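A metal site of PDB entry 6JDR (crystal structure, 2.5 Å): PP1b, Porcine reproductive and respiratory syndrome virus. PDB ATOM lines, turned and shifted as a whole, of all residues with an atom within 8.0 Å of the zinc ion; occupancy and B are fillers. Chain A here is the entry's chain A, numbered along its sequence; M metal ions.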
ATOM      1  N   TYR A   9     -21.813 -13.253 -24.195  1.00  0.00           N
ATOM      2  CA  TYR A   9     -21.341 -12.511 -25.367  1.00  0.00           C
ATOM      3  C   TYR A   9     -20.873 -11.113 -24.979  1.00  0.00           C
ATOM      4  O   TYR A   9     -19.699 -10.755 -25.190  1.00  0.00           O
ATOM      5  CB  TYR A   9     -22.441 -12.374 -26.412  1.00  0.00           C
ATOM      6  CG  TYR A   9     -22.862 -13.654 -27.103  1.00  0.00           C
ATOM      7  CD1 TYR A   9     -21.987 -14.322 -27.962  1.00  0.00           C
ATOM      8  CD2 TYR A   9     -24.128 -14.192 -26.923  1.00  0.00           C
ATOM      9  CE1 TYR A   9     -22.364 -15.484 -28.606  1.00  0.00           C
ATOM     10  CE2 TYR A   9     -24.520 -15.345 -27.569  1.00  0.00           C
ATOM     11  CZ  TYR A   9     -23.630 -15.995 -28.409  1.00  0.00           C
ATOM     12  OH  TYR A   9     -24.007 -17.156 -29.053  1.00  0.00           O
ATOM     13  N   ALA A  17     -30.740 -18.262 -20.845  1.00  0.00           N
ATOM     14  CA  ALA A  17     -29.548 -19.051 -21.128  1.00  0.00           C
ATOM     15  C   ALA A  17     -29.783 -20.017 -22.286  1.00  0.00           C
ATOM     16  O   ALA A  17     -30.918 -20.419 -22.554  1.00  0.00           O
ATOM     17  CB  ALA A  17     -29.136 -19.832 -19.890  1.00  0.00           C
ATOM     18  N   THR A  18     -28.695 -20.374 -22.975  1.00  0.00           N
ATOM     19  CA  THR A  18     -28.758 -21.382 -24.037  1.00  0.00           C
ATOM     20  C   THR A  18     -28.788 -22.758 -23.402  1.00  0.00           C
ATOM     21  O   THR A  18     -28.371 -22.927 -22.258  1.00  0.00           O
ATOM     22  CB  THR A  18     -27.544 -21.304 -25.005  1.00  0.00           C
ATOM     23  OG1 THR A  18     -26.347 -21.700 -24.325  1.00  0.00           O
ATOM     24  CG2 THR A  18     -27.383 -19.887 -25.550  1.00  0.00           C
ATOM     25  N   ALA A  19     -29.286 -23.734 -24.156  1.00  0.00           N
ATOM     26  CA  ALA A  19     -29.301 -25.115 -23.692  1.00  0.00           C
ATOM     27  C   ALA A  19     -27.898 -25.661 -23.436  1.00  0.00           C
ATOM     28  O   ALA A  19     -27.713 -26.574 -22.647  1.00  0.00           O
ATOM     29  CB  ALA A  19     -30.038 -25.997 -24.694  1.00  0.00           C
ATOM     30  N   CYS A  20     -26.906 -25.080 -24.122  1.00  0.00           N
ATOM     31  CA  CYS A  20     -25.502 -25.479 -23.946  1.00  0.00           C
ATOM     32  C   CYS A  20     -24.779 -24.713 -22.826  1.00  0.00           C
ATOM     33  O   CYS A  20     -23.551 -24.788 -22.725  1.00  0.00           O
ATOM     34  CB  CYS A  20     -24.754 -25.335 -25.270  1.00  0.00           C
ATOM     35  SG  CYS A  20     -24.445 -23.628 -25.771  1.00  0.00           S
ATOM     36  N   GLY A  21     -25.517 -23.987 -21.994  1.00  0.00           N
ATOM     37  CA  GLY A  21     -24.972 -23.412 -20.755  1.00  0.00           C
ATOM     38  C   GLY A  21     -24.470 -21.975 -20.817  1.00  0.00           C
ATOM     39  O   GLY A  21     -23.858 -21.501 -19.869  1.00  0.00           O
ATOM     40  N   LEU A  22     -24.756 -21.276 -21.918  1.00  0.00           N
ATOM     41  CA  LEU A  22     -24.315 -19.886 -22.075  1.00  0.00           C
ATOM     42  C   LEU A  22     -25.402 -18.923 -21.594  1.00  0.00           C
ATOM     43  O   LEU A  22     -26.521 -18.956 -22.105  1.00  0.00           O
ATOM     44  CB  LEU A  22     -23.990 -19.604 -23.550  1.00  0.00           C
ATOM     45  CG  LEU A  22     -23.261 -18.290 -23.839  1.00  0.00           C
ATOM     46  CD1 LEU A  22     -21.814 -18.338 -23.366  1.00  0.00           C
ATOM     47  CD2 LEU A  22     -23.311 -17.976 -25.327  1.00  0.00           C
ATOM     48  N   HIS A  32     -28.193 -17.154 -31.507  1.00  0.00           N
ATOM     49  CA  HIS A  32     -27.491 -18.362 -31.077  1.00  0.00           C
ATOM     50  C   HIS A  32     -28.107 -19.565 -31.769  1.00  0.00           C
ATOM     51  O   HIS A  32     -29.008 -20.212 -31.236  1.00  0.00           O
ATOM     52  CB  HIS A  32     -27.564 -18.494 -29.562  1.00  0.00           C
ATOM     53  CG  HIS A  32     -26.719 -19.592 -29.003  1.00  0.00           C
ATOM     54  ND1 HIS A  32     -25.418 -19.396 -28.592  1.00  0.00           N
ATOM     55  CD2 HIS A  32     -26.998 -20.895 -28.764  1.00  0.00           C
ATOM     56  CE1 HIS A  32     -24.927 -20.538 -28.141  1.00  0.00           C
ATOM     57  NE2 HIS A  32     -25.874 -21.455 -28.225  1.00  0.00           N
ATOM     58  N   GLN A  33     -27.607 -19.876 -32.956  1.00  0.00           N
ATOM     59  CA  GLN A  33     -28.182 -20.929 -33.792  1.00  0.00           C
ATOM     60  C   GLN A  33     -27.701 -22.325 -33.388  1.00  0.00           C
ATOM     61  O   GLN A  33     -28.230 -23.322 -33.881  1.00  0.00           O
ATOM     62  CB  GLN A  33     -27.875 -20.657 -35.267  1.00  0.00           C
ATOM     63  CG  GLN A  33     -28.390 -19.313 -35.742  1.00  0.00           C
ATOM     64  CD  GLN A  33     -28.241 -19.108 -37.238  1.00  0.00           C
ATOM     65  OE1 GLN A  33     -27.261 -19.529 -37.840  1.00  0.00           O
ATOM     66  NE2 GLN A  33     -29.216 -18.452 -37.846  1.00  0.00           N
ATOM     67  N   HIS A  34     -26.707 -22.383 -32.514  1.00  0.00           N
ATOM     68  CA  HIS A  34     -26.131 -23.647 -32.035  1.00  0.00           C
ATOM     69  C   HIS A  34     -27.141 -24.576 -31.368  1.00  0.00           C
ATOM     70  O   HIS A  34     -27.126 -25.782 -31.589  1.00  0.00           O
ATOM     71  CB  HIS A  34     -24.990 -23.335 -31.066  1.00  0.00           C
ATOM     72  CG  HIS A  34     -24.367 -24.543 -30.444  1.00  0.00           C
ATOM     73  ND1 HIS A  34     -24.478 -24.817 -29.094  1.00  0.00           N
ATOM     74  CD2 HIS A  34     -23.621 -25.542 -30.969  1.00  0.00           C
ATOM     75  CE1 HIS A  34     -23.840 -25.939 -28.822  1.00  0.00           C
ATOM     76  NE2 HIS A  34     -23.306 -26.399 -29.942  1.00  0.00           N
ATOM     77  N   CYS A  35     -28.022 -24.013 -30.550  1.00  0.00           N
ATOM     78  CA  CYS A  35     -28.971 -24.807 -29.780  1.00  0.00           C
ATOM     79  C   CYS A  35     -30.123 -23.938 -29.287  1.00  0.00           C
ATOM     80  O   CYS A  35     -30.044 -22.711 -29.375  1.00  0.00           O
ATOM     81  CB  CYS A  35     -28.261 -25.496 -28.608  1.00  0.00           C
ATOM     82  SG  CYS A  35     -27.646 -24.360 -27.347  1.00  0.00           S
ATOM     83  N   PRO A  36     -31.205 -24.562 -28.783  1.00  0.00           N
ATOM     84  CA  PRO A  36     -32.362 -23.779 -28.355  1.00  0.00           C
ATOM     85  C   PRO A  36     -32.095 -22.770 -27.231  1.00  0.00           C
ATOM     86  O   PRO A  36     -31.280 -23.026 -26.331  1.00  0.00           O
ATOM     87  CB  PRO A  36     -33.345 -24.849 -27.851  1.00  0.00           C
ATOM     88  CG  PRO A  36     -32.964 -26.084 -28.590  1.00  0.00           C
ATOM     89  CD  PRO A  36     -31.477 -26.012 -28.728  1.00  0.00           C
ATOM     90  N   VAL A  37     -32.783 -21.640 -27.305  1.00  0.00           N
ATOM     91  CA  VAL A  37     -32.794 -20.661 -26.233  1.00  0.00           C
ATOM     92  C   VAL A  37     -34.252 -20.424 -25.820  1.00  0.00           C
ATOM     93  O   VAL A  37     -35.008 -19.771 -26.537  1.00  0.00           O
ATOM     94  CB  VAL A  37     -32.163 -19.324 -26.671  1.00  0.00           C
ATOM     95  CG1 VAL A  37     -32.101 -18.348 -25.504  1.00  0.00           C
ATOM     96  CG2 VAL A  37     -30.778 -19.569 -27.249  1.00  0.00           C
ATOM     97  N   LEU A  64     -17.329 -16.978 -31.150  1.00  0.00           N
ATOM     98  CA  LEU A  64     -17.846 -18.126 -30.411  1.00  0.00           C
ATOM     99  C   LEU A  64     -18.823 -18.935 -31.250  1.00  0.00           C
ATOM    100  O   LEU A  64     -18.817 -20.157 -31.204  1.00  0.00           O
ATOM    101  CB  LEU A  64     -18.560 -17.669 -29.136  1.00  0.00           C
ATOM    102  CG  LEU A  64     -19.162 -18.765 -28.256  1.00  0.00           C
ATOM    103  CD1 LEU A  64     -18.080 -19.690 -27.712  1.00  0.00           C
ATOM    104  CD2 LEU A  64     -19.959 -18.155 -27.114  1.00  0.00           C
ATOM    105  N   ASP A  65     -19.648 -18.236 -32.011  1.00  0.00           N
ATOM    106  CA  ASP A  65     -20.687 -18.890 -32.790  1.00  0.00           C
ATOM    107  C   ASP A  65     -20.072 -19.695 -33.927  1.00  0.00           C
ATOM    108  O   ASP A  65     -20.580 -20.762 -34.273  1.00  0.00           O
ATOM    109  CB  ASP A  65     -21.673 -17.841 -33.316  1.00  0.00           C
ATOM    110  CG  ASP A  65     -22.300 -17.037 -32.200  1.00  0.00           C
ATOM    111  OD1 ASP A  65     -22.830 -17.662 -31.256  1.00  0.00           O
ATOM    112  OD2 ASP A  65     -22.243 -15.783 -32.250  1.00  0.00           O
ATOM    113  N   LEU A  68     -18.620 -22.805 -32.372  1.00  0.00           N
ATOM    114  CA  LEU A  68     -19.680 -23.736 -31.999  1.00  0.00           C
ATOM    115  C   LEU A  68     -20.281 -24.529 -33.169  1.00  0.00           C
ATOM    116  O   LEU A  68     -20.984 -25.495 -32.941  1.00  0.00           O
ATOM    117  CB  LEU A  68     -20.793 -23.025 -31.222  1.00  0.00           C
ATOM    118  CG  LEU A  68     -20.472 -22.586 -29.788  1.00  0.00           C
ATOM    119  CD1 LEU A  68     -21.606 -21.746 -29.232  1.00  0.00           C
ATOM    120  CD2 LEU A  68     -20.179 -23.772 -28.890  1.00  0.00           C
ATOM    121  N   VAL A  71     -19.363 -27.996 -32.729  1.00  0.00           N
ATOM    122  CA  VAL A  71     -19.708 -28.547 -31.420  1.00  0.00           C
ATOM    123  C   VAL A  71     -21.171 -29.026 -31.440  1.00  0.00           C
ATOM    124  O   VAL A  71     -22.083 -28.214 -31.347  1.00  0.00           O
ATOM    125  CB  VAL A  71     -19.493 -27.502 -30.303  1.00  0.00           C
ATOM    126  CG1 VAL A  71     -19.708 -28.129 -28.930  1.00  0.00           C
ATOM    127  CG2 VAL A  71     -18.095 -26.907 -30.396  1.00  0.00           C
ATOM    128  N   PRO A  72     -21.395 -30.350 -31.597  1.00  0.00           N
ATOM    129  CA  PRO A  72     -22.755 -30.905 -31.668  1.00  0.00           C
ATOM    130  C   PRO A  72     -23.565 -30.727 -30.387  1.00  0.00           C
ATOM    131  O   PRO A  72     -23.074 -31.030 -29.307  1.00  0.00           O
ATOM    132  CB  PRO A  72     -22.527 -32.405 -31.896  1.00  0.00           C
ATOM    133  CG  PRO A  72     -21.122 -32.541 -32.362  1.00  0.00           C
ATOM    134  CD  PRO A  72     -20.367 -31.386 -31.803  1.00  0.00           C
ATOM    135  N   TYR A  73     -24.796 -30.243 -30.523  1.00  0.00           N
ATOM    136  CA  TYR A  73     -25.718 -30.196 -29.411  1.00  0.00           C
ATOM    137  C   TYR A  73     -26.476 -31.521 -29.343  1.00  0.00           C
ATOM    138  O   TYR A  73     -27.163 -31.890 -30.294  1.00  0.00           O
ATOM    139  CB  TYR A  73     -26.704 -29.034 -29.539  1.00  0.00           C
ATOM    140  CG  TYR A  73     -27.796 -29.078 -28.495  1.00  0.00           C
ATOM    141  CD1 TYR A  73     -27.480 -28.999 -27.141  1.00  0.00           C
ATOM    142  CD2 TYR A  73     -29.132 -29.221 -28.858  1.00  0.00           C
ATOM    143  CE1 TYR A  73     -28.471 -29.053 -26.179  1.00  0.00           C
ATOM    144  CE2 TYR A  73     -30.133 -29.279 -27.895  1.00  0.00           C
ATOM    145  CZ  TYR A  73     -29.786 -29.196 -26.563  1.00  0.00           C
ATOM    146  OH  TYR A  73     -30.765 -29.252 -25.594  1.00  0.00           O
ATOM    147  N   LEU A 126     -26.441 -28.058 -20.488  1.00  0.00           N
ATOM    148  CA  LEU A 126     -25.160 -28.745 -20.664  1.00  0.00           C
ATOM    149  C   LEU A 126     -24.023 -27.870 -20.154  1.00  0.00           C
ATOM    150  O   LEU A 126     -24.161 -26.636 -20.068  1.00  0.00           O
ATOM    151  CB  LEU A 126     -24.941 -29.085 -22.138  1.00  0.00           C
ATOM    152  CG  LEU A 126     -25.962 -30.029 -22.786  1.00  0.00           C
ATOM    153  CD1 LEU A 126     -25.767 -30.098 -24.289  1.00  0.00           C
ATOM    154  CD2 LEU A 126     -25.862 -31.425 -22.189  1.00  0.00           C
ATOM    155  N   THR A 128     -21.293 -27.313 -21.745  1.00  0.00           N
ATOM    156  CA  THR A 128     -20.502 -26.854 -22.895  1.00  0.00           C
ATOM    157  C   THR A 128     -19.955 -25.437 -22.724  1.00  0.00           C
ATOM    158  O   THR A 128     -18.737 -25.241 -22.794  1.00  0.00           O
ATOM    159  CB  THR A 128     -21.309 -26.909 -24.198  1.00  0.00           C
ATOM    160  OG1 THR A 128     -22.015 -28.155 -24.299  1.00  0.00           O
ATOM    161  CG2 THR A 128     -20.382 -26.754 -25.420  1.00  0.00           C
ATOM    162  N   CYS A 129     -20.833 -24.474 -22.497  1.00  0.00           N
ATOM    163  CA  CYS A 129     -20.429 -23.067 -22.392  1.00  0.00           C
ATOM    164  C   CYS A 129     -20.620 -22.499 -20.980  1.00  0.00           C
ATOM    165  O   CYS A 129     -20.753 -21.289 -20.812  1.00  0.00           O
ATOM    166  CB  CYS A 129     -21.185 -22.224 -23.410  1.00  0.00           C
ATOM    167  SG  CYS A 129     -20.770 -22.602 -25.133  1.00  0.00           S
HETATM  168 ZN    ZN M   1     -25.576 -23.531 -27.741  1.00  0.00          ZN
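ND1 of His 32 lies within hydrogen-bond range of OH of Tyr 9, at 2.7 Å. O of Val 71 sits at hydrogen-bond distance from NE2 of His 34 (2.6 Å). SG of Cys 35 lies close to N of Ala 19. N of Cys 20 lies close to OG1 of Thr 18 (3.4 Å). O of Cys 20 lies within hydrogen-bond range of N of Cys 129. The side-chain hydroxyl of Thr 18 lies within hydrogen-bond range of the backbone NH of Gly 21, 3.4 Å away. OG1 of Thr 18 sits at hydrogen-bond distance from N of Leu 22 (2.9 Å).
Thr 18 touches the zinc ion. Of the 22 residues printed, 5 come within 4 Å of the zinc ion. Along chain A the residues within 4 Å of the zinc ion span positions 18 to 35.
The zinc ion is bound by NE2 of His 32 (2.2 Å), ND1 of His 34 (2.2 Å), SG of Cys 35 (2.3 Å) and SG of Cys 20 (2.3 Å). The zinc ion has four donor atoms within binding distance.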
